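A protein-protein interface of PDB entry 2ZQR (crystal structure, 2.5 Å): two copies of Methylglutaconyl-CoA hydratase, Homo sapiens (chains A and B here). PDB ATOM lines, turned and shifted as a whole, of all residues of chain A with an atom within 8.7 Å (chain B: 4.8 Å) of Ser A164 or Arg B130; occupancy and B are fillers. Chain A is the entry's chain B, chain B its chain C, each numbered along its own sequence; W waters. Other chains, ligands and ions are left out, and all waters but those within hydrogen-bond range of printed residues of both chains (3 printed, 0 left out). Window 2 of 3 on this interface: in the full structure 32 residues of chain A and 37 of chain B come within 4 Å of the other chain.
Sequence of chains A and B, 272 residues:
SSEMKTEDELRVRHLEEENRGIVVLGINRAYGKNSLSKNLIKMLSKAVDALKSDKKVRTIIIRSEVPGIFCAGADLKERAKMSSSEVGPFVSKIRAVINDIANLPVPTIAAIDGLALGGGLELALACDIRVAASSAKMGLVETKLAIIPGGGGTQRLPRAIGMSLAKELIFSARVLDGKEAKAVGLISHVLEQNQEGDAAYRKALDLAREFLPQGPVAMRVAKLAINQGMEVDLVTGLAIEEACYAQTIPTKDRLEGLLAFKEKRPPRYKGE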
ATOM      1  N   LEU A 157      11.532   8.404  -6.116  1.00  0.00           N
ATOM      2  CA  LEU A 157      12.124   9.469  -6.900  1.00  0.00           C
ATOM      3  C   LEU A 157      13.510   9.870  -6.422  1.00  0.00           C
ATOM      4  O   LEU A 157      14.435   9.965  -7.220  1.00  0.00           O
ATOM      5  CB  LEU A 157      11.212  10.696  -6.939  1.00  0.00           C
ATOM      6  CG  LEU A 157      11.732  11.772  -7.894  1.00  0.00           C
ATOM      7  CD1 LEU A 157      11.912  11.146  -9.282  1.00  0.00           C
ATOM      8  CD2 LEU A 157      10.783  12.958  -7.942  1.00  0.00           C
ATOM      9  N   PRO A 158      13.677  10.113  -5.113  1.00  0.00           N
ATOM     10  CA  PRO A 158      14.990  10.504  -4.585  1.00  0.00           C
ATOM     11  C   PRO A 158      15.995   9.360  -4.682  1.00  0.00           C
ATOM     12  O   PRO A 158      17.192   9.581  -4.843  1.00  0.00           O
ATOM     13  CB  PRO A 158      14.687  10.867  -3.131  1.00  0.00           C
ATOM     14  CG  PRO A 158      13.228  11.227  -3.152  1.00  0.00           C
ATOM     15  CD  PRO A 158      12.657  10.173  -4.053  1.00  0.00           C
ATOM     16  N   ARG A 159      15.492   8.137  -4.568  1.00  0.00           N
ATOM     17  CA  ARG A 159      16.337   6.956  -4.639  1.00  0.00           C
ATOM     18  C   ARG A 159      16.931   6.815  -6.030  1.00  0.00           C
ATOM     19  O   ARG A 159      18.124   6.543  -6.174  1.00  0.00           O
ATOM     20  CB  ARG A 159      15.532   5.704  -4.270  1.00  0.00           C
ATOM     21  CG  ARG A 159      15.409   5.514  -2.776  1.00  0.00           C
ATOM     22  CD  ARG A 159      14.443   4.415  -2.415  1.00  0.00           C
ATOM     23  NE  ARG A 159      14.520   4.093  -0.992  1.00  0.00           N
ATOM     24  CZ  ARG A 159      14.057   4.865  -0.013  1.00  0.00           C
ATOM     25  NH1 ARG A 159      13.464   6.026  -0.281  1.00  0.00           N
ATOM     26  NH2 ARG A 159      14.188   4.469   1.241  1.00  0.00           N
ATOM     27  N   ILE A 161      16.954   9.352  -8.673  1.00  0.00           N
ATOM     28  CA  ILE A 161      17.704  10.493  -9.206  1.00  0.00           C
ATOM     29  C   ILE A 161      18.425  11.338  -8.168  1.00  0.00           C
ATOM     30  O   ILE A 161      19.066  12.335  -8.510  1.00  0.00           O
ATOM     31  CB  ILE A 161      16.792  11.442 -10.043  1.00  0.00           C
ATOM     32  CG1 ILE A 161      15.910  12.286  -9.117  1.00  0.00           C
ATOM     33  CG2 ILE A 161      15.931  10.623 -11.001  1.00  0.00           C
ATOM     34  CD1 ILE A 161      15.030  13.282  -9.841  1.00  0.00           C
ATOM     35  N   GLY A 162      18.334  10.944  -6.903  1.00  0.00           N
ATOM     36  CA  GLY A 162      18.991  11.718  -5.865  1.00  0.00           C
ATOM     37  C   GLY A 162      18.031  12.677  -5.182  1.00  0.00           C
ATOM     38  O   GLY A 162      17.055  13.138  -5.778  1.00  0.00           O
ATOM     39  N   MET A 163      18.316  12.985  -3.924  1.00  0.00           N
ATOM     40  CA  MET A 163      17.475  13.873  -3.133  1.00  0.00           C
ATOM     41  C   MET A 163      17.230  15.241  -3.754  1.00  0.00           C
ATOM     42  O   MET A 163      16.084  15.639  -3.975  1.00  0.00           O
ATOM     43  CB  MET A 163      18.095  14.076  -1.752  1.00  0.00           C
ATOM     44  CG  MET A 163      17.301  13.501  -0.611  1.00  0.00           C
ATOM     45  SD  MET A 163      17.829  14.296   0.910  1.00  0.00           S
ATOM     46  CE  MET A 163      19.383  13.415   1.257  1.00  0.00           C
ATOM     47  N   SER A 164      18.315  15.959  -4.023  1.00  0.00           N
ATOM     48  CA  SER A 164      18.233  17.308  -4.576  1.00  0.00           C
ATOM     49  C   SER A 164      17.313  17.419  -5.788  1.00  0.00           C
ATOM     50  O   SER A 164      16.290  18.111  -5.747  1.00  0.00           O
ATOM     51  CB  SER A 164      19.634  17.803  -4.937  1.00  0.00           C
ATOM     52  OG  SER A 164      19.676  19.216  -4.911  1.00  0.00           O
ATOM     53  N   LEU A 165      17.688  16.729  -6.862  1.00  0.00           N
ATOM     54  CA  LEU A 165      16.923  16.726  -8.096  1.00  0.00           C
ATOM     55  C   LEU A 165      15.477  16.285  -7.867  1.00  0.00           C
ATOM     56  O   LEU A 165      14.559  16.796  -8.514  1.00  0.00           O
ATOM     57  CB  LEU A 165      17.598  15.806  -9.117  1.00  0.00           C
ATOM     58  CG  LEU A 165      18.983  16.242  -9.613  1.00  0.00           C
ATOM     59  CD1 LEU A 165      19.621  15.129 -10.446  1.00  0.00           C
ATOM     60  CD2 LEU A 165      18.846  17.522 -10.431  1.00  0.00           C
ATOM     61  N   ALA A 166      15.270  15.330  -6.961  1.00  0.00           N
ATOM     62  CA  ALA A 166      13.918  14.854  -6.681  1.00  0.00           C
ATOM     63  C   ALA A 166      13.131  15.927  -5.913  1.00  0.00           C
ATOM     64  O   ALA A 166      11.963  16.184  -6.215  1.00  0.00           O
ATOM     65  CB  ALA A 166      13.971  13.559  -5.891  1.00  0.00           C
ATOM     66  N   LYS A 167      13.771  16.558  -4.930  1.00  0.00           N
ATOM     67  CA  LYS A 167      13.104  17.605  -4.164  1.00  0.00           C
ATOM     68  C   LYS A 167      12.661  18.731  -5.102  1.00  0.00           C
ATOM     69  O   LYS A 167      11.483  19.086  -5.153  1.00  0.00           O
ATOM     70  CB  LYS A 167      14.031  18.166  -3.080  1.00  0.00           C
ATOM     71  CG  LYS A 167      14.261  17.245  -1.881  1.00  0.00           C
ATOM     72  CD  LYS A 167      15.325  17.840  -0.958  1.00  0.00           C
ATOM     73  CE  LYS A 167      15.449  17.080   0.364  1.00  0.00           C
ATOM     74  NZ  LYS A 167      16.569  17.609   1.210  1.00  0.00           N
ATOM     75  N   GLU A 168      13.602  19.279  -5.861  1.00  0.00           N
ATOM     76  CA  GLU A 168      13.274  20.359  -6.780  1.00  0.00           C
ATOM     77  C   GLU A 168      12.047  20.022  -7.620  1.00  0.00           C
ATOM     78  O   GLU A 168      11.121  20.825  -7.724  1.00  0.00           O
ATOM     79  CB  GLU A 168      14.461  20.668  -7.702  1.00  0.00           C
ATOM     80  CG  GLU A 168      14.187  21.831  -8.642  1.00  0.00           C
ATOM     81  CD  GLU A 168      15.406  22.278  -9.420  1.00  0.00           C
ATOM     82  OE1 GLU A 168      16.491  22.391  -8.812  1.00  0.00           O
ATOM     83  OE2 GLU A 168      15.271  22.530 -10.637  1.00  0.00           O
ATOM     84  N   LEU A 169      12.032  18.832  -8.213  1.00  0.00           N
ATOM     85  CA  LEU A 169      10.905  18.426  -9.045  1.00  0.00           C
ATOM     86  C   LEU A 169       9.581  18.407  -8.288  1.00  0.00           C
ATOM     87  O   LEU A 169       8.553  18.814  -8.830  1.00  0.00           O
ATOM     88  CB  LEU A 169      11.181  17.055  -9.675  1.00  0.00           C
ATOM     89  CG  LEU A 169      12.293  17.072 -10.738  1.00  0.00           C
ATOM     90  CD1 LEU A 169      12.564  15.668 -11.270  1.00  0.00           C
ATOM     91  CD2 LEU A 169      11.872  18.004 -11.880  1.00  0.00           C
ATOM     92  N   ILE A 170       9.609  17.953  -7.034  1.00  0.00           N
ATOM     93  CA  ILE A 170       8.395  17.891  -6.221  1.00  0.00           C
ATOM     94  C   ILE A 170       7.959  19.282  -5.749  1.00  0.00           C
ATOM     95  O   ILE A 170       6.767  19.601  -5.737  1.00  0.00           O
ATOM     96  CB  ILE A 170       8.589  17.019  -4.960  1.00  0.00           C
ATOM     97  CG1 ILE A 170       9.191  15.666  -5.326  1.00  0.00           C
ATOM     98  CG2 ILE A 170       7.251  16.804  -4.281  1.00  0.00           C
ATOM     99  CD1 ILE A 170       8.315  14.827  -6.203  1.00  0.00           C
ATOM    100  N   PHE A 171       8.932  20.093  -5.342  1.00  0.00           N
ATOM    101  CA  PHE A 171       8.668  21.439  -4.854  1.00  0.00           C
ATOM    102  C   PHE A 171       8.137  22.308  -5.975  1.00  0.00           C
ATOM    103  O   PHE A 171       7.249  23.131  -5.754  1.00  0.00           O
ATOM    104  CB  PHE A 171       9.946  22.092  -4.315  1.00  0.00           C
ATOM    105  CG  PHE A 171      10.511  21.447  -3.078  1.00  0.00           C
ATOM    106  CD1 PHE A 171      11.824  21.723  -2.688  1.00  0.00           C
ATOM    107  CD2 PHE A 171       9.750  20.578  -2.301  1.00  0.00           C
ATOM    108  CE1 PHE A 171      12.375  21.144  -1.545  1.00  0.00           C
ATOM    109  CE2 PHE A 171      10.291  19.986  -1.145  1.00  0.00           C
ATOM    110  CZ  PHE A 171      11.606  20.272  -0.770  1.00  0.00           C
ATOM    111  N   ALA B 110      20.786  27.180  -1.669  1.00  0.00           N
ATOM    112  CA  ALA B 110      22.074  27.767  -1.340  1.00  0.00           C
ATOM    113  C   ALA B 110      22.643  28.454  -2.579  1.00  0.00           C
ATOM    114  O   ALA B 110      23.018  27.785  -3.546  1.00  0.00           O
ATOM    115  CB  ALA B 110      23.021  26.680  -0.868  1.00  0.00           C
ATOM    116  N   ILE B 112      25.531  30.073  -4.348  1.00  0.00           N
ATOM    117  CA  ILE B 112      26.986  30.164  -4.213  1.00  0.00           C
ATOM    118  C   ILE B 112      27.665  31.038  -5.271  1.00  0.00           C
ATOM    119  O   ILE B 112      27.916  30.603  -6.397  1.00  0.00           O
ATOM    120  CB  ILE B 112      27.642  28.764  -4.245  1.00  0.00           C
ATOM    121  CG1 ILE B 112      26.980  27.841  -3.220  1.00  0.00           C
ATOM    122  CG2 ILE B 112      29.123  28.888  -3.932  1.00  0.00           C
ATOM    123  CD1 ILE B 112      27.498  26.409  -3.272  1.00  0.00           C
ATOM    124  N   ALA B 124      26.016  24.502   2.566  1.00  0.00           N
ATOM    125  CA  ALA B 124      25.278  24.386   1.311  1.00  0.00           C
ATOM    126  C   ALA B 124      24.694  22.987   1.114  1.00  0.00           C
ATOM    127  O   ALA B 124      23.579  22.830   0.613  1.00  0.00           O
ATOM    128  CB  ALA B 124      26.193  24.761   0.122  1.00  0.00           C
ATOM    129  N   LEU B 125      25.450  21.968   1.505  1.00  0.00           N
ATOM    130  CA  LEU B 125      24.978  20.599   1.374  1.00  0.00           C
ATOM    131  C   LEU B 125      23.735  20.399   2.250  1.00  0.00           C
ATOM    132  O   LEU B 125      22.880  19.559   1.943  1.00  0.00           O
ATOM    133  CB  LEU B 125      26.093  19.620   1.762  1.00  0.00           C
ATOM    134  CG  LEU B 125      27.276  19.543   0.777  1.00  0.00           C
ATOM    135  CD1 LEU B 125      28.505  18.917   1.455  1.00  0.00           C
ATOM    136  CD2 LEU B 125      26.863  18.738  -0.457  1.00  0.00           C
ATOM    137  N   CYS B 127      21.402  22.408   2.475  1.00  0.00           N
ATOM    138  CA  CYS B 127      20.275  23.005   1.759  1.00  0.00           C
ATOM    139  C   CYS B 127      19.766  21.948   0.793  1.00  0.00           C
ATOM    140  O   CYS B 127      20.473  20.987   0.492  1.00  0.00           O
ATOM    141  CB  CYS B 127      20.708  24.257   0.989  1.00  0.00           C
ATOM    142  SG  CYS B 127      21.185  25.646   2.048  1.00  0.00           S
ATOM    143  N   ASP B 128      18.541  22.126   0.321  1.00  0.00           N
ATOM    144  CA  ASP B 128      17.920  21.188  -0.600  1.00  0.00           C
ATOM    145  C   ASP B 128      18.459  21.273  -2.027  1.00  0.00           C
ATOM    146  O   ASP B 128      18.673  20.245  -2.682  1.00  0.00           O
ATOM    147  CB  ASP B 128      16.413  21.419  -0.629  1.00  0.00           C
ATOM    148  CG  ASP B 128      15.772  21.208   0.713  1.00  0.00           C
ATOM    149  OD1 ASP B 128      16.351  20.438   1.504  1.00  0.00           O
ATOM    150  OD2 ASP B 128      14.692  21.796   0.971  1.00  0.00           O
ATOM    151  N   ILE B 129      18.662  22.508  -2.489  1.00  0.00           N
ATOM    152  CA  ILE B 129      19.146  22.796  -3.833  1.00  0.00           C
ATOM    153  C   ILE B 129      20.393  23.681  -3.776  1.00  0.00           C
ATOM    154  O   ILE B 129      20.471  24.599  -2.963  1.00  0.00           O
ATOM    155  CB  ILE B 129      18.107  23.597  -4.629  1.00  0.00           C
ATOM    156  CG1 ILE B 129      16.694  23.057  -4.377  1.00  0.00           C
ATOM    157  CG2 ILE B 129      18.497  23.611  -6.102  1.00  0.00           C
ATOM    158  CD1 ILE B 129      16.374  21.786  -5.097  1.00  0.00           C
ATOM    159  N   ARG B 130      21.351  23.425  -4.659  1.00  0.00           N
ATOM    160  CA  ARG B 130      22.578  24.215  -4.726  1.00  0.00           C
ATOM    161  C   ARG B 130      22.739  24.853  -6.110  1.00  0.00           C
ATOM    162  O   ARG B 130      22.670  24.172  -7.131  1.00  0.00           O
ATOM    163  CB  ARG B 130      23.794  23.339  -4.403  1.00  0.00           C
ATOM    164  CG  ARG B 130      24.085  23.210  -2.912  1.00  0.00           C
ATOM    165  CD  ARG B 130      25.052  22.072  -2.593  1.00  0.00           C
ATOM    166  NE  ARG B 130      24.541  20.774  -3.037  1.00  0.00           N
ATOM    167  CZ  ARG B 130      23.421  20.211  -2.595  1.00  0.00           C
ATOM    168  NH1 ARG B 130      22.676  20.815  -1.676  1.00  0.00           N
ATOM    169  NH2 ARG B 130      23.022  19.057  -3.101  1.00  0.00           N
ATOM    170  N   VAL B 131      22.931  26.170  -6.130  1.00  0.00           N
ATOM    171  CA  VAL B 131      23.115  26.914  -7.373  1.00  0.00           C
ATOM    172  C   VAL B 131      24.393  27.736  -7.262  1.00  0.00           C
ATOM    173  O   VAL B 131      24.563  28.506  -6.317  1.00  0.00           O
ATOM    174  CB  VAL B 131      21.933  27.859  -7.643  1.00  0.00           C
ATOM    175  CG1 VAL B 131      20.647  27.068  -7.644  1.00  0.00           C
ATOM    176  CG2 VAL B 131      21.873  28.945  -6.587  1.00  0.00           C
ATOM    177  N   ALA B 132      25.295  27.572  -8.223  1.00  0.00           N
ATOM    178  CA  ALA B 132      26.556  28.298  -8.180  1.00  0.00           C
ATOM    179  C   ALA B 132      27.013  28.820  -9.528  1.00  0.00           C
ATOM    180  O   ALA B 132      26.539  28.378 -10.573  1.00  0.00           O
ATOM    181  CB  ALA B 132      27.646  27.413  -7.584  1.00  0.00           C
ATOM    182  N   ALA B 160      25.337  12.951  -1.709  1.00  0.00           N
ATOM    183  CA  ALA B 160      25.019  13.843  -2.821  1.00  0.00           C
ATOM    184  C   ALA B 160      25.691  13.531  -4.166  1.00  0.00           C
ATOM    185  O   ALA B 160      25.055  13.644  -5.214  1.00  0.00           O
ATOM    186  CB  ALA B 160      25.321  15.291  -2.411  1.00  0.00           C
ATOM    187  N   LEU B 186      27.531  17.957  -7.698  1.00  0.00           N
ATOM    188  CA  LEU B 186      27.554  18.687  -6.434  1.00  0.00           C
ATOM    189  C   LEU B 186      26.499  19.803  -6.388  1.00  0.00           C
ATOM    190  O   LEU B 186      25.967  20.122  -5.321  1.00  0.00           O
ATOM    191  CB  LEU B 186      28.943  19.276  -6.198  1.00  0.00           C
ATOM    192  CG  LEU B 186      29.179  19.926  -4.831  1.00  0.00           C
ATOM    193  CD1 LEU B 186      28.956  18.897  -3.724  1.00  0.00           C
ATOM    194  CD2 LEU B 186      30.601  20.489  -4.762  1.00  0.00           C
ATOM    195  N   ILE B 187      26.212  20.407  -7.540  1.00  0.00           N
ATOM    196  CA  ILE B 187      25.195  21.455  -7.619  1.00  0.00           C
ATOM    197  C   ILE B 187      24.199  21.091  -8.719  1.00  0.00           C
ATOM    198  O   ILE B 187      24.511  20.293  -9.597  1.00  0.00           O
ATOM    199  CB  ILE B 187      25.812  22.857  -7.910  1.00  0.00           C
ATOM    200  CG1 ILE B 187      26.555  22.844  -9.246  1.00  0.00           C
ATOM    201  CG2 ILE B 187      26.740  23.260  -6.770  1.00  0.00           C
ATOM    202  CD1 ILE B 187      27.223  24.157  -9.602  1.00  0.00           C
ATOM    203  N   SER B 188      23.003  21.674  -8.671  1.00  0.00           N
ATOM    204  CA  SER B 188      21.973  21.374  -9.658  1.00  0.00           C
ATOM    205  C   SER B 188      21.799  22.456 -10.720  1.00  0.00           C
ATOM    206  O   SER B 188      21.094  22.258 -11.697  1.00  0.00           O
ATOM    207  CB  SER B 188      20.640  21.147  -8.945  1.00  0.00           C
ATOM    208  OG  SER B 188      20.804  20.246  -7.865  1.00  0.00           O
ATOM    209  N   HIS B 189      22.436  23.600 -10.515  1.00  0.00           N
ATOM    210  CA  HIS B 189      22.346  24.724 -11.442  1.00  0.00           C
ATOM    211  C   HIS B 189      23.652  25.491 -11.411  1.00  0.00           C
ATOM    212  O   HIS B 189      24.140  25.860 -10.343  1.00  0.00           O
ATOM    213  CB  HIS B 189      21.205  25.656 -11.037  1.00  0.00           C
ATOM    214  CG  HIS B 189      19.874  24.979 -10.981  1.00  0.00           C
ATOM    215  ND1 HIS B 189      19.170  24.633 -12.113  1.00  0.00           N
ATOM    216  CD2 HIS B 189      19.149  24.523  -9.932  1.00  0.00           C
ATOM    217  CE1 HIS B 189      18.068  23.993 -11.765  1.00  0.00           C
ATOM    218  NE2 HIS B 189      18.032  23.912 -10.447  1.00  0.00           N
HETATM  219  O   HOH W   1      17.613  19.104   3.641  1.00  0.00           O
HETATM  220  O   HOH W   2      21.499  21.179  -5.692  1.00  0.00           O
HETATM  221  O   HOH W   3      18.662  17.627  -0.628  1.00  0.00           O
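Of the 15 printed residues of chain B, 5 touch a printed residue of chain A.
Along chain B the printed residues that touch a printed residue of chain A span positions 128 to 189.
Of the 14 printed residues of chain A, 4 touch a printed residue of chain B.
Water W2 lies within hydrogen-bond range of the side-chain hydroxyl (OG) of Ser B188 (2.5 Å), the backbone NH (N) of Arg B130 (2.5 Å) and the side-chain hydroxyl (OG) of Ser A164 (2.8 Å).
Water W3 lies within hydrogen-bond range of the side-chain amino group (NZ) of Lys A167 (2.8 Å), the backbone carbonyl oxygen (O) of Asp B128 (3.3 Å) and the side-chain sulfur (SD) of Met A163 (3.8 Å).
Water W1 lies within hydrogen-bond range of the side-chain carboxylate (OD1) of Asp B128 (2.8 Å) and the side-chain amino group (NZ) of Lys A167 (3.0 Å).
No position is printed for both chains.
The side-chain hydroxyl (OG) of Ser A164 sits at hydrogen-bond distance from the backbone carbonyl oxygen (O) of Asp B128, at 2.7 Å.
The side-chain hydroxyl (OG) of Ser A164 sits at hydrogen-bond distance from the side-chain hydroxyl (OG) of Ser B188, at 3.3 Å.
The side-chain amino group (NZ) of Lys A167 lies within salt-bridge range of the side-chain carboxylate (OD1) of Asp B128.
NE2 of His B189 lies within hydrogen-bond range of OE1 of Glu A168 (2.7 Å).
Ile B129 touches Ser A164 (CD1 to O, 3.7 Å).
NH2 of Arg B130 touches OG of Ser A164, 3.8 Å away.
CB of Glu A168 touches CD1 of Ile B129 (3.4 Å).
Asp B128 touches Phe A171.
Ser A164 touches four residues of chain B.
Printed residues of chain B within 4 Å of Phe A171: Asp B128.
Ile B112 touches none of the printed residues of chain A.
Of chain A, only Ser A164 comes within 4 Å of Arg B130.
Ala B160 touches none of the printed residues of chain A.
Of the printed residues of chain A, Ser B188 touches Ser A164 (3.3 Å).
The nearest printed residue of chain A that does not touch Ile B129 is Lys A167 (4.8 Å).
The side-chain sulfur of Met A163 lies within hydrogen-bond range of the side-chain amino group of Lys A167 (3.6 Å).
The backbone carbonyl oxygen of Ile B129 sits at hydrogen-bond distance from the backbone NH of Ala B110 (2.9 Å).
O of Cys B127 sits at hydrogen-bond distance from NH1 of Arg B130 (3.1 Å).
The guanidinium group (NE) of Arg B130 lies within hydrogen-bond range of the backbone carbonyl oxygen (O) of Leu B186 (2.8 Å).
The backbone carbonyl oxygen of Arg B130 lies within hydrogen-bond range of the backbone NH of Ser B188 (3.0 Å).
N of Ala B132 lies within hydrogen-bond range of O of His B189, 3.0 Å away.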
